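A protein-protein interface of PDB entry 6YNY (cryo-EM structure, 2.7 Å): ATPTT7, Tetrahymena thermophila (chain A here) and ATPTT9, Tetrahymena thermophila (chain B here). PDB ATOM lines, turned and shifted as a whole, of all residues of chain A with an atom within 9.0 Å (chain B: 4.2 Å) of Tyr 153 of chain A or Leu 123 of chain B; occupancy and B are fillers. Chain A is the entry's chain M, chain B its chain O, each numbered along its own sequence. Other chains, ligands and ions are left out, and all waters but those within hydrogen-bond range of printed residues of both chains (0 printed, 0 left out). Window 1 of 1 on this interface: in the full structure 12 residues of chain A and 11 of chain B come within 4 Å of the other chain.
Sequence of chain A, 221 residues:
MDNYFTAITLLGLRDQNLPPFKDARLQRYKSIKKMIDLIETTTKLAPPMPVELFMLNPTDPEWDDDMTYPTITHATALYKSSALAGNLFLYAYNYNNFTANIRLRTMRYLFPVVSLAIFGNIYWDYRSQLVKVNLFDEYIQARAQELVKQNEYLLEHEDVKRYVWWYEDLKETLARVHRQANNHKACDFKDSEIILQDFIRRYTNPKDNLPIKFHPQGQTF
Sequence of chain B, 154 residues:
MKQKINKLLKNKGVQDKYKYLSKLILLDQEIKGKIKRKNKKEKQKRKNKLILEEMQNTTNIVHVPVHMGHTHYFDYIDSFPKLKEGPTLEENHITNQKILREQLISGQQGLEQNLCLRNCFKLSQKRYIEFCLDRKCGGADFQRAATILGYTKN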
ATOM      1  N   PRO A  50       9.759   5.933 -25.114  1.00  0.00           N
ATOM      2  CA  PRO A  50      10.833   6.814 -25.588  1.00  0.00           C
ATOM      3  C   PRO A  50      12.201   6.160 -25.463  1.00  0.00           C
ATOM      4  O   PRO A  50      12.582   5.676 -24.397  1.00  0.00           O
ATOM      5  CB  PRO A  50      10.710   8.041 -24.683  1.00  0.00           C
ATOM      6  CG  PRO A  50       9.311   8.034 -24.229  1.00  0.00           C
ATOM      7  CD  PRO A  50       8.918   6.601 -24.108  1.00  0.00           C
ATOM      8  N   VAL A  51      12.941   6.146 -26.573  1.00  0.00           N
ATOM      9  CA  VAL A  51      14.295   5.608 -26.541  1.00  0.00           C
ATOM     10  C   VAL A  51      15.206   6.494 -25.705  1.00  0.00           C
ATOM     11  O   VAL A  51      16.189   6.015 -25.128  1.00  0.00           O
ATOM     12  CB  VAL A  51      14.846   5.438 -27.968  1.00  0.00           C
ATOM     13  CG1 VAL A  51      13.997   4.472 -28.754  1.00  0.00           C
ATOM     14  CG2 VAL A  51      14.929   6.773 -28.675  1.00  0.00           C
ATOM     15  N   GLU A  52      14.907   7.786 -25.623  1.00  0.00           N
ATOM     16  CA  GLU A  52      15.718   8.723 -24.848  1.00  0.00           C
ATOM     17  C   GLU A  52      15.288   8.742 -23.388  1.00  0.00           C
ATOM     18  O   GLU A  52      15.050   9.791 -22.795  1.00  0.00           O
ATOM     19  CB  GLU A  52      15.628  10.117 -25.455  1.00  0.00           C
ATOM     20  CG  GLU A  52      15.897  10.175 -26.943  1.00  0.00           C
ATOM     21  CD  GLU A  52      14.661   9.899 -27.776  1.00  0.00           C
ATOM     22  OE1 GLU A  52      13.650   9.432 -27.212  1.00  0.00           O
ATOM     23  OE2 GLU A  52      14.700  10.155 -28.998  1.00  0.00           O
ATOM     24  N   LEU A  53      15.207   7.556 -22.797  1.00  0.00           N
ATOM     25  CA  LEU A  53      14.765   7.373 -21.424  1.00  0.00           C
ATOM     26  C   LEU A  53      15.877   6.870 -20.520  1.00  0.00           C
ATOM     27  O   LEU A  53      16.137   7.456 -19.466  1.00  0.00           O
ATOM     28  CB  LEU A  53      13.589   6.392 -21.402  1.00  0.00           C
ATOM     29  CG  LEU A  53      12.479   6.605 -20.381  1.00  0.00           C
ATOM     30  CD1 LEU A  53      11.854   7.966 -20.550  1.00  0.00           C
ATOM     31  CD2 LEU A  53      11.438   5.529 -20.554  1.00  0.00           C
ATOM     32  N   MET A  55      18.934   6.028 -22.160  1.00  0.00           N
ATOM     33  CA  MET A  55      20.010   5.972 -23.141  1.00  0.00           C
ATOM     34  C   MET A  55      20.056   7.286 -23.897  1.00  0.00           C
ATOM     35  O   MET A  55      19.074   7.661 -24.544  1.00  0.00           O
ATOM     36  CB  MET A  55      19.793   4.803 -24.092  1.00  0.00           C
ATOM     37  CG  MET A  55      20.649   4.821 -25.325  1.00  0.00           C
ATOM     38  SD  MET A  55      20.524   3.281 -26.233  1.00  0.00           S
ATOM     39  CE  MET A  55      21.119   3.822 -27.819  1.00  0.00           C
ATOM     40  N   LEU A  56      21.186   7.978 -23.815  1.00  0.00           N
ATOM     41  CA  LEU A  56      21.376   9.196 -24.585  1.00  0.00           C
ATOM     42  C   LEU A  56      21.592   8.858 -26.051  1.00  0.00           C
ATOM     43  O   LEU A  56      22.232   7.859 -26.387  1.00  0.00           O
ATOM     44  CB  LEU A  56      22.567   9.983 -24.049  1.00  0.00           C
ATOM     45  CG  LEU A  56      22.427  10.539 -22.638  1.00  0.00           C
ATOM     46  CD1 LEU A  56      23.747  11.063 -22.148  1.00  0.00           C
ATOM     47  CD2 LEU A  56      21.393  11.631 -22.600  1.00  0.00           C
ATOM     48  N   ASN A  57      21.058   9.694 -26.922  1.00  0.00           N
ATOM     49  CA  ASN A  57      21.182   9.451 -28.350  1.00  0.00           C
ATOM     50  C   ASN A  57      22.640   9.570 -28.768  1.00  0.00           C
ATOM     51  O   ASN A  57      23.217  10.660 -28.662  1.00  0.00           O
ATOM     52  CB  ASN A  57      20.325  10.428 -29.132  1.00  0.00           C
ATOM     53  CG  ASN A  57      20.146  10.012 -30.572  1.00  0.00           C
ATOM     54  OD1 ASN A  57      21.090   9.582 -31.231  1.00  0.00           O
ATOM     55  ND2 ASN A  57      18.924  10.123 -31.065  1.00  0.00           N
ATOM     56  N   THR A  59      23.900   9.705 -31.655  1.00  0.00           N
ATOM     57  CA  THR A  59      24.048  10.485 -32.874  1.00  0.00           C
ATOM     58  C   THR A  59      24.002  11.984 -32.623  1.00  0.00           C
ATOM     59  O   THR A  59      24.049  12.761 -33.583  1.00  0.00           O
ATOM     60  CB  THR A  59      22.952  10.112 -33.875  1.00  0.00           C
ATOM     61  OG1 THR A  59      21.698  10.640 -33.431  1.00  0.00           O
ATOM     62  CG2 THR A  59      22.836   8.611 -34.003  1.00  0.00           C
ATOM     63  N   ASP A  60      23.911  12.409 -31.370  1.00  0.00           N
ATOM     64  CA  ASP A  60      23.834  13.825 -31.070  1.00  0.00           C
ATOM     65  C   ASP A  60      25.181  14.494 -31.338  1.00  0.00           C
ATOM     66  O   ASP A  60      26.231  13.914 -31.047  1.00  0.00           O
ATOM     67  CB  ASP A  60      23.415  14.033 -29.616  1.00  0.00           C
ATOM     68  CG  ASP A  60      23.204  15.490 -29.266  1.00  0.00           C
ATOM     69  OD1 ASP A  60      24.138  16.296 -29.447  1.00  0.00           O
ATOM     70  OD2 ASP A  60      22.096  15.830 -28.806  1.00  0.00           O
ATOM     71  N   LEU A 147      21.925  16.674 -17.836  1.00  0.00           N
ATOM     72  CA  LEU A 147      21.115  15.945 -18.801  1.00  0.00           C
ATOM     73  C   LEU A 147      19.960  15.216 -18.134  1.00  0.00           C
ATOM     74  O   LEU A 147      18.921  14.998 -18.765  1.00  0.00           O
ATOM     75  CB  LEU A 147      21.991  14.965 -19.570  1.00  0.00           C
ATOM     76  CG  LEU A 147      23.026  15.627 -20.472  1.00  0.00           C
ATOM     77  CD1 LEU A 147      24.009  14.614 -20.990  1.00  0.00           C
ATOM     78  CD2 LEU A 147      22.343  16.333 -21.622  1.00  0.00           C
ATOM     79  N   VAL A 148      20.121  14.824 -16.873  1.00  0.00           N
ATOM     80  CA  VAL A 148      19.029  14.179 -16.153  1.00  0.00           C
ATOM     81  C   VAL A 148      17.896  15.168 -15.923  1.00  0.00           C
ATOM     82  O   VAL A 148      16.760  14.948 -16.357  1.00  0.00           O
ATOM     83  CB  VAL A 148      19.537  13.586 -14.829  1.00  0.00           C
ATOM     84  CG1 VAL A 148      18.385  13.086 -14.000  1.00  0.00           C
ATOM     85  CG2 VAL A 148      20.493  12.461 -15.098  1.00  0.00           C
ATOM     86  N   LYS A 149      18.191  16.281 -15.250  1.00  0.00           N
ATOM     87  CA  LYS A 149      17.178  17.304 -15.026  1.00  0.00           C
ATOM     88  C   LYS A 149      16.528  17.760 -16.322  1.00  0.00           C
ATOM     89  O   LYS A 149      15.397  18.257 -16.298  1.00  0.00           O
ATOM     90  CB  LYS A 149      17.797  18.514 -14.324  1.00  0.00           C
ATOM     91  CG  LYS A 149      18.264  18.251 -12.913  1.00  0.00           C
ATOM     92  CD  LYS A 149      18.697  19.535 -12.227  1.00  0.00           C
ATOM     93  CE  LYS A 149      20.000  20.078 -12.792  1.00  0.00           C
ATOM     94  NZ  LYS A 149      21.149  19.174 -12.516  1.00  0.00           N
ATOM     95  N   GLN A 150      17.214  17.597 -17.450  1.00  0.00           N
ATOM     96  CA  GLN A 150      16.675  18.032 -18.729  1.00  0.00           C
ATOM     97  C   GLN A 150      15.659  17.051 -19.296  1.00  0.00           C
ATOM     98  O   GLN A 150      14.692  17.475 -19.936  1.00  0.00           O
ATOM     99  CB  GLN A 150      17.820  18.235 -19.720  1.00  0.00           C
ATOM    100  CG  GLN A 150      17.397  18.490 -21.149  1.00  0.00           C
ATOM    101  CD  GLN A 150      18.577  18.679 -22.072  1.00  0.00           C
ATOM    102  OE1 GLN A 150      18.645  18.080 -23.143  1.00  0.00           O
ATOM    103  NE2 GLN A 150      19.516  19.518 -21.663  1.00  0.00           N
ATOM    104  N   ASN A 151      15.853  15.750 -19.077  1.00  0.00           N
ATOM    105  CA  ASN A 151      15.017  14.726 -19.688  1.00  0.00           C
ATOM    106  C   ASN A 151      14.181  13.955 -18.673  1.00  0.00           C
ATOM    107  O   ASN A 151      13.641  12.895 -18.999  1.00  0.00           O
ATOM    108  CB  ASN A 151      15.893  13.773 -20.496  1.00  0.00           C
ATOM    109  CG  ASN A 151      16.569  14.456 -21.658  1.00  0.00           C
ATOM    110  OD1 ASN A 151      16.054  15.429 -22.208  1.00  0.00           O
ATOM    111  ND2 ASN A 151      17.730  13.953 -22.042  1.00  0.00           N
ATOM    112  N   GLU A 152      14.057  14.467 -17.448  1.00  0.00           N
ATOM    113  CA  GLU A 152      13.199  13.823 -16.461  1.00  0.00           C
ATOM    114  C   GLU A 152      11.746  13.785 -16.914  1.00  0.00           C
ATOM    115  O   GLU A 152      11.019  12.841 -16.589  1.00  0.00           O
ATOM    116  CB  GLU A 152      13.306  14.549 -15.121  1.00  0.00           C
ATOM    117  CG  GLU A 152      14.475  14.121 -14.275  1.00  0.00           C
ATOM    118  CD  GLU A 152      14.606  14.937 -13.006  1.00  0.00           C
ATOM    119  OE1 GLU A 152      14.095  16.075 -12.974  1.00  0.00           O
ATOM    120  OE2 GLU A 152      15.218  14.440 -12.037  1.00  0.00           O
ATOM    121  N   TYR A 153      11.308  14.800 -17.662  1.00  0.00           N
ATOM    122  CA  TYR A 153       9.902  14.905 -18.031  1.00  0.00           C
ATOM    123  C   TYR A 153       9.434  13.721 -18.867  1.00  0.00           C
ATOM    124  O   TYR A 153       8.240  13.404 -18.872  1.00  0.00           O
ATOM    125  CB  TYR A 153       9.666  16.208 -18.791  1.00  0.00           C
ATOM    126  CG  TYR A 153      10.343  16.259 -20.136  1.00  0.00           C
ATOM    127  CD1 TYR A 153       9.668  15.892 -21.287  1.00  0.00           C
ATOM    128  CD2 TYR A 153      11.655  16.673 -20.254  1.00  0.00           C
ATOM    129  CE1 TYR A 153      10.281  15.936 -22.513  1.00  0.00           C
ATOM    130  CE2 TYR A 153      12.276  16.720 -21.476  1.00  0.00           C
ATOM    131  CZ  TYR A 153      11.586  16.350 -22.602  1.00  0.00           C
ATOM    132  OH  TYR A 153      12.210  16.400 -23.823  1.00  0.00           O
ATOM    133  N   LEU A 154      10.346  13.057 -19.575  1.00  0.00           N
ATOM    134  CA  LEU A 154       9.945  11.964 -20.453  1.00  0.00           C
ATOM    135  C   LEU A 154       9.286  10.824 -19.694  1.00  0.00           C
ATOM    136  O   LEU A 154       8.560  10.029 -20.302  1.00  0.00           O
ATOM    137  CB  LEU A 154      11.153  11.443 -21.223  1.00  0.00           C
ATOM    138  CG  LEU A 154      11.735  12.400 -22.258  1.00  0.00           C
ATOM    139  CD1 LEU A 154      13.035  11.859 -22.817  1.00  0.00           C
ATOM    140  CD2 LEU A 154      10.741  12.639 -23.372  1.00  0.00           C
ATOM    141  N   LEU A 155       9.517  10.721 -18.390  1.00  0.00           N
ATOM    142  CA  LEU A 155       8.879   9.694 -17.583  1.00  0.00           C
ATOM    143  C   LEU A 155       7.432  10.022 -17.248  1.00  0.00           C
ATOM    144  O   LEU A 155       6.723   9.155 -16.728  1.00  0.00           O
ATOM    145  CB  LEU A 155       9.669   9.481 -16.293  1.00  0.00           C
ATOM    146  CG  LEU A 155      11.089   8.953 -16.484  1.00  0.00           C
ATOM    147  CD1 LEU A 155      11.839   8.973 -15.179  1.00  0.00           C
ATOM    148  CD2 LEU A 155      11.065   7.556 -17.044  1.00  0.00           C
ATOM    149  N   GLU A 156       6.984  11.241 -17.531  1.00  0.00           N
ATOM    150  CA  GLU A 156       5.602  11.637 -17.319  1.00  0.00           C
ATOM    151  C   GLU A 156       4.715  11.348 -18.521  1.00  0.00           C
ATOM    152  O   GLU A 156       3.500  11.553 -18.440  1.00  0.00           O
ATOM    153  CB  GLU A 156       5.535  13.127 -16.987  1.00  0.00           C
ATOM    154  CG  GLU A 156       6.301  13.521 -15.747  1.00  0.00           C
ATOM    155  CD  GLU A 156       6.327  15.021 -15.534  1.00  0.00           C
ATOM    156  OE1 GLU A 156       5.853  15.756 -16.425  1.00  0.00           O
ATOM    157  OE2 GLU A 156       6.820  15.464 -14.477  1.00  0.00           O
ATOM    158  N   HIS A 157       5.287  10.883 -19.626  1.00  0.00           N
ATOM    159  CA  HIS A 157       4.502  10.617 -20.819  1.00  0.00           C
ATOM    160  C   HIS A 157       3.615   9.396 -20.612  1.00  0.00           C
ATOM    161  O   HIS A 157       3.986   8.437 -19.931  1.00  0.00           O
ATOM    162  CB  HIS A 157       5.419  10.404 -22.019  1.00  0.00           C
ATOM    163  CG  HIS A 157       4.743  10.601 -23.339  1.00  0.00           C
ATOM    164  ND1 HIS A 157       4.176   9.565 -24.046  1.00  0.00           N
ATOM    165  CD2 HIS A 157       4.550  11.715 -24.084  1.00  0.00           C
ATOM    166  CE1 HIS A 157       3.659  10.031 -25.167  1.00  0.00           C
ATOM    167  NE2 HIS A 157       3.872  11.333 -25.214  1.00  0.00           N
ATOM    168  N   GLU A 158       2.425   9.442 -21.208  1.00  0.00           N
ATOM    169  CA  GLU A 158       1.459   8.370 -21.020  1.00  0.00           C
ATOM    170  C   GLU A 158       1.912   7.064 -21.655  1.00  0.00           C
ATOM    171  O   GLU A 158       1.385   6.004 -21.304  1.00  0.00           O
ATOM    172  CB  GLU A 158       0.105   8.789 -21.588  1.00  0.00           C
ATOM    173  CG  GLU A 158      -1.038   7.869 -21.210  1.00  0.00           C
ATOM    174  CD  GLU A 158      -2.371   8.349 -21.739  1.00  0.00           C
ATOM    175  OE1 GLU A 158      -2.378   9.190 -22.662  1.00  0.00           O
ATOM    176  OE2 GLU A 158      -3.413   7.892 -21.226  1.00  0.00           O
ATOM    177  N   VAL A 160       4.647   5.578 -21.151  1.00  0.00           N
ATOM    178  CA  VAL A 160       5.261   4.764 -20.110  1.00  0.00           C
ATOM    179  C   VAL A 160       4.195   3.972 -19.373  1.00  0.00           C
ATOM    180  O   VAL A 160       4.389   2.798 -19.039  1.00  0.00           O
ATOM    181  CB  VAL A 160       6.072   5.648 -19.148  1.00  0.00           C
ATOM    182  CG1 VAL A 160       6.658   4.812 -18.037  1.00  0.00           C
ATOM    183  CG2 VAL A 160       7.163   6.376 -19.891  1.00  0.00           C
ATOM    184  N   GLN A 217      10.384   1.210 -34.140  1.00  0.00           N
ATOM    185  CA  GLN A 217      10.509   0.999 -32.704  1.00  0.00           C
ATOM    186  C   GLN A 217       9.658  -0.168 -32.223  1.00  0.00           C
ATOM    187  O   GLN A 217       9.161  -0.153 -31.093  1.00  0.00           O
ATOM    188  CB  GLN A 217      10.138   2.276 -31.956  1.00  0.00           C
ATOM    189  CG  GLN A 217      10.728   2.375 -30.573  1.00  0.00           C
ATOM    190  CD  GLN A 217      10.454   3.705 -29.919  1.00  0.00           C
ATOM    191  OE1 GLN A 217      10.153   4.691 -30.588  1.00  0.00           O
ATOM    192  NE2 GLN A 217      10.550   3.739 -28.600  1.00  0.00           N
ATOM    193  N   CYS B 120      14.640  19.871 -27.946  1.00  0.00           N
ATOM    194  CA  CYS B 120      13.387  19.152 -28.131  1.00  0.00           C
ATOM    195  C   CYS B 120      13.321  18.501 -29.505  1.00  0.00           C
ATOM    196  O   CYS B 120      12.801  17.389 -29.646  1.00  0.00           O
ATOM    197  CB  CYS B 120      12.204  20.099 -27.937  1.00  0.00           C
ATOM    198  SG  CYS B 120      11.919  20.681 -26.244  1.00  0.00           S
ATOM    199  N   PHE B 121      13.841  19.173 -30.531  1.00  0.00           N
ATOM    200  CA  PHE B 121      13.789  18.643 -31.886  1.00  0.00           C
ATOM    201  C   PHE B 121      14.791  17.526 -32.137  1.00  0.00           C
ATOM    202  O   PHE B 121      14.752  16.915 -33.209  1.00  0.00           O
ATOM    203  CB  PHE B 121      14.023  19.762 -32.898  1.00  0.00           C
ATOM    204  CG  PHE B 121      12.781  20.495 -33.286  1.00  0.00           C
ATOM    205  CD1 PHE B 121      12.086  20.144 -34.425  1.00  0.00           C
ATOM    206  CD2 PHE B 121      12.306  21.535 -32.514  1.00  0.00           C
ATOM    207  CE1 PHE B 121      10.945  20.815 -34.784  1.00  0.00           C
ATOM    208  CE2 PHE B 121      11.165  22.209 -32.871  1.00  0.00           C
ATOM    209  CZ  PHE B 121      10.483  21.849 -34.006  1.00  0.00           C
ATOM    210  N   LYS B 122      15.685  17.249 -31.194  1.00  0.00           N
ATOM    211  CA  LYS B 122      16.625  16.147 -31.319  1.00  0.00           C
ATOM    212  C   LYS B 122      16.047  14.831 -30.823  1.00  0.00           C
ATOM    213  O   LYS B 122      16.787  13.849 -30.701  1.00  0.00           O
ATOM    214  CB  LYS B 122      17.915  16.468 -30.565  1.00  0.00           C
ATOM    215  CG  LYS B 122      18.745  17.548 -31.219  1.00  0.00           C
ATOM    216  CD  LYS B 122      20.168  17.604 -30.694  1.00  0.00           C
ATOM    217  CE  LYS B 122      20.249  18.157 -29.285  1.00  0.00           C
ATOM    218  NZ  LYS B 122      19.843  17.166 -28.251  1.00  0.00           N
ATOM    219  N   LEU B 123      14.751  14.789 -30.535  1.00  0.00           N
ATOM    220  CA  LEU B 123      14.116  13.570 -30.076  1.00  0.00           C
ATOM    221  C   LEU B 123      13.737  12.683 -31.259  1.00  0.00           C
ATOM    222  O   LEU B 123      13.736  13.104 -32.417  1.00  0.00           O
ATOM    223  CB  LEU B 123      12.890  13.902 -29.231  1.00  0.00           C
ATOM    224  CG  LEU B 123      13.205  14.667 -27.946  1.00  0.00           C
ATOM    225  CD1 LEU B 123      11.946  15.051 -27.226  1.00  0.00           C
ATOM    226  CD2 LEU B 123      14.081  13.843 -27.034  1.00  0.00           C
ATOM    227  N   SER B 124      13.403  11.433 -30.943  1.00  0.00           N
ATOM    228  CA  SER B 124      13.183  10.432 -31.979  1.00  0.00           C
ATOM    229  C   SER B 124      11.853  10.649 -32.688  1.00  0.00           C
ATOM    230  O   SER B 124      11.803  10.805 -33.912  1.00  0.00           O
ATOM    231  CB  SER B 124      13.245   9.035 -31.364  1.00  0.00           C
ATOM    232  OG  SER B 124      12.328   8.904 -30.293  1.00  0.00           O
ATOM    233  N   GLN B 125      10.763  10.658 -31.933  1.00  0.00           N
ATOM    234  CA  GLN B 125       9.423  10.737 -32.492  1.00  0.00           C
ATOM    235  C   GLN B 125       8.869  12.151 -32.375  1.00  0.00           C
ATOM    236  O   GLN B 125       9.297  12.948 -31.539  1.00  0.00           O
ATOM    237  CB  GLN B 125       8.491   9.752 -31.790  1.00  0.00           C
ATOM    238  CG  GLN B 125       8.963   8.319 -31.855  1.00  0.00           C
ATOM    239  CD  GLN B 125       8.978   7.776 -33.262  1.00  0.00           C
ATOM    240  OE1 GLN B 125       8.515   8.425 -34.197  1.00  0.00           O
ATOM    241  NE2 GLN B 125       9.512   6.576 -33.420  1.00  0.00           N
ATOM    242  N   TYR B 128       6.924  13.065 -29.093  1.00  0.00           N
ATOM    243  CA  TYR B 128       7.774  13.422 -27.965  1.00  0.00           C
ATOM    244  C   TYR B 128       8.282  14.852 -28.077  1.00  0.00           C
ATOM    245  O   TYR B 128       8.534  15.498 -27.055  1.00  0.00           O
ATOM    246  CB  TYR B 128       8.953  12.455 -27.872  1.00  0.00           C
ATOM    247  CG  TYR B 128       8.561  11.005 -27.739  1.00  0.00           C
ATOM    248  CD1 TYR B 128       9.349  10.007 -28.280  1.00  0.00           C
ATOM    249  CD2 TYR B 128       7.407  10.632 -27.070  1.00  0.00           C
ATOM    250  CE1 TYR B 128       9.000   8.683 -28.168  1.00  0.00           C
ATOM    251  CE2 TYR B 128       7.051   9.311 -26.952  1.00  0.00           C
ATOM    252  CZ  TYR B 128       7.850   8.339 -27.501  1.00  0.00           C
ATOM    253  OH  TYR B 128       7.496   7.016 -27.383  1.00  0.00           O
ATOM    254  N   ILE B 129       8.439  15.357 -29.300  1.00  0.00           N
ATOM    255  CA  ILE B 129       8.841  16.746 -29.486  1.00  0.00           C
ATOM    256  C   ILE B 129       7.757  17.681 -28.973  1.00  0.00           C
ATOM    257  O   ILE B 129       8.027  18.615 -28.209  1.00  0.00           O
ATOM    258  CB  ILE B 129       9.155  17.017 -30.966  1.00  0.00           C
ATOM    259  CG1 ILE B 129      10.298  16.122 -31.439  1.00  0.00           C
ATOM    260  CG2 ILE B 129       9.500  18.475 -31.168  1.00  0.00           C
ATOM    261  CD1 ILE B 129      10.555  16.186 -32.916  1.00  0.00           C
ATOM    262  N   PHE B 131       5.561  17.095 -26.809  1.00  0.00           N
ATOM    263  CA  PHE B 131       5.547  16.996 -25.357  1.00  0.00           C
ATOM    264  C   PHE B 131       6.678  17.809 -24.743  1.00  0.00           C
ATOM    265  O   PHE B 131       6.499  18.445 -23.698  1.00  0.00           O
ATOM    266  CB  PHE B 131       5.646  15.526 -24.958  1.00  0.00           C
ATOM    267  CG  PHE B 131       5.449  15.271 -23.498  1.00  0.00           C
ATOM    268  CD1 PHE B 131       4.191  15.340 -22.936  1.00  0.00           C
ATOM    269  CD2 PHE B 131       6.517  14.932 -22.692  1.00  0.00           C
ATOM    270  CE1 PHE B 131       4.006  15.097 -21.597  1.00  0.00           C
ATOM    271  CE2 PHE B 131       6.336  14.685 -21.354  1.00  0.00           C
ATOM    272  CZ  PHE B 131       5.079  14.767 -20.806  1.00  0.00           C
ATOM    273  N   CYS B 132       7.847  17.807 -25.384  1.00  0.00           N
ATOM    274  CA  CYS B 132       8.971  18.595 -24.892  1.00  0.00           C
ATOM    275  C   CYS B 132       8.691  20.088 -25.007  1.00  0.00           C
ATOM    276  O   CYS B 132       8.981  20.853 -24.081  1.00  0.00           O
ATOM    277  CB  CYS B 132      10.233  18.217 -25.665  1.00  0.00           C
ATOM    278  SG  CYS B 132      11.774  18.992 -25.124  1.00  0.00           S
ATOM    279  N   ARG B 135       6.001  21.054 -22.410  1.00  0.00           N
ATOM    280  CA  ARG B 135       6.427  20.851 -21.032  1.00  0.00           C
ATOM    281  C   ARG B 135       7.620  21.720 -20.652  1.00  0.00           C
ATOM    282  O   ARG B 135       7.679  22.225 -19.527  1.00  0.00           O
ATOM    283  CB  ARG B 135       6.762  19.376 -20.815  1.00  0.00           C
ATOM    284  CG  ARG B 135       7.366  19.048 -19.463  1.00  0.00           C
ATOM    285  CD  ARG B 135       6.466  19.482 -18.322  1.00  0.00           C
ATOM    286  NE  ARG B 135       7.055  19.185 -17.021  1.00  0.00           N
ATOM    287  CZ  ARG B 135       6.462  19.434 -15.857  1.00  0.00           C
ATOM    288  NH1 ARG B 135       5.257  19.988 -15.821  1.00  0.00           N
ATOM    289  NH2 ARG B 135       7.078  19.126 -14.725  1.00  0.00           N
ATOM    290  N   LYS B 136       8.573  21.909 -21.562  1.00  0.00           N
ATOM    291  CA  LYS B 136       9.810  22.621 -21.263  1.00  0.00           C
ATOM    292  C   LYS B 136       9.886  24.007 -21.879  1.00  0.00           C
ATOM    293  O   LYS B 136      10.426  24.920 -21.254  1.00  0.00           O
ATOM    294  CB  LYS B 136      11.012  21.805 -21.749  1.00  0.00           C
ATOM    295  CG  LYS B 136      11.077  20.389 -21.210  1.00  0.00           C
ATOM    296  CD  LYS B 136      11.265  20.338 -19.703  1.00  0.00           C
ATOM    297  CE  LYS B 136      12.584  20.947 -19.270  1.00  0.00           C
ATOM    298  NZ  LYS B 136      13.734  20.365 -20.001  1.00  0.00           N
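The side-chain hydroxyl (OH) of Tyr 128 of chain B sits close to the backbone nitrogen (N) of Pro 50 of chain A (3.4 Å).
The side-chain hydroxyl of Tyr 153 of chain A sits at hydrogen-bond distance from the side-chain sulfur of Cys 132 of chain B (2.9 Å).
The side-chain carboxylate (OE2) of Glu 156 of chain A lies within salt-bridge range of the guanidinium group (NH2) of Arg 135 of chain B (3.7 Å).
NZ of Lys 122 of chain B lies within salt-bridge range of OD2 of Asp 60 of chain A (2.7 Å).
O of Gln 150 of chain A lies within hydrogen-bond range of NZ of Lys 136 of chain B (3.0 Å).
OE1 of Gln 217 of chain A sits at hydrogen-bond distance from NE2 of Gln 125 of chain B (3.5 Å).
The side-chain carboxylate (OE2) of Glu 52 of chain A is in hydrogen-bond range of the backbone NH (N) of Ser 124 of chain B (2.7 Å).
The side-chain sulfur (SG) of Cys 120 of chain B forms a disulfide with the side-chain sulfur (SG) of Cys 132 of chain B, 2.0 Å away.
Among the printed residues, pairs that only touch across the chains: Val 51 of chain A with Ser 124 of chain B (3.7 Å), Glu 52 of chain A with Leu 123 of chain B (3.5 Å), Tyr 153 of chain A with Leu 123 of chain B (3.7 Å), Tyr 153 of chain A with Phe 131 of chain B (3.4 Å), Tyr 153 of chain A with Arg 135 of chain B (3.7 Å), Tyr 153 of chain A with Lys 136 of chain B (3.7 Å), His 157 of chain A with Tyr 128 of chain B (3.9 Å) and His 157 of chain A with Phe 131 of chain B (3.7 Å).
Of chain A, only Glu 52 (3.5 Å) and Tyr 153 (3.7 Å) come within 4 Å of Leu 123 of chain B.
Of the printed residues of chain A, Ser 124 of chain B touches Val 51 (3.7 Å) and Glu 52 (2.7 Å).
Of the printed residues of chain B, Glu 52 of chain A touches Leu 123 and Ser 124.
Printed residues of chain A within 4 Å of Gln 125 of chain B: Gln 217 (3.5 Å).
Of the printed residues of chain B, Asp 60 of chain A touches Lys 122 (2.7 Å).
Of the printed residues of chain B, Gln 150 of chain A touches Lys 136 (3.0 Å).
Lys 149 of chain A touches none of the printed residues of chain B.
The nearest printed residue of chain B that does not touch Tyr 153 of chain A is Tyr 128 of chain B (4.9 Å).
The nearest printed residue of chain B that does not touch Glu 52 of chain A is Tyr 128 of chain B (4.5 Å).
Of the 23 printed residues of chain A, 9 touch a printed residue of chain B.
Hydrophobic or aromatic side chains of chain A that line the printed part of chain B: Pro 50, Val 51, Tyr 153 and His 157.
Printed residues of chain B that touch a printed residue of chain A: Lys 122, Leu 123, Ser 124, Gln 125, Tyr 128, Phe 131, Cys 132, Arg 135 and Lys 136.
Hydrophobic or aromatic side chains of chain B that line the printed part of chain A: Leu 123, Tyr 128 and Phe 131.
Among the printed residues, Asp or Glu carboxylates within 4 Å of a Lys or Arg side-chain nitrogen of the other chain: Asp 60 of chain A with Lys 122 of chain B (2.7 Å) and Glu 156 of chain A with Arg 135 of chain B (3.7 Å).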
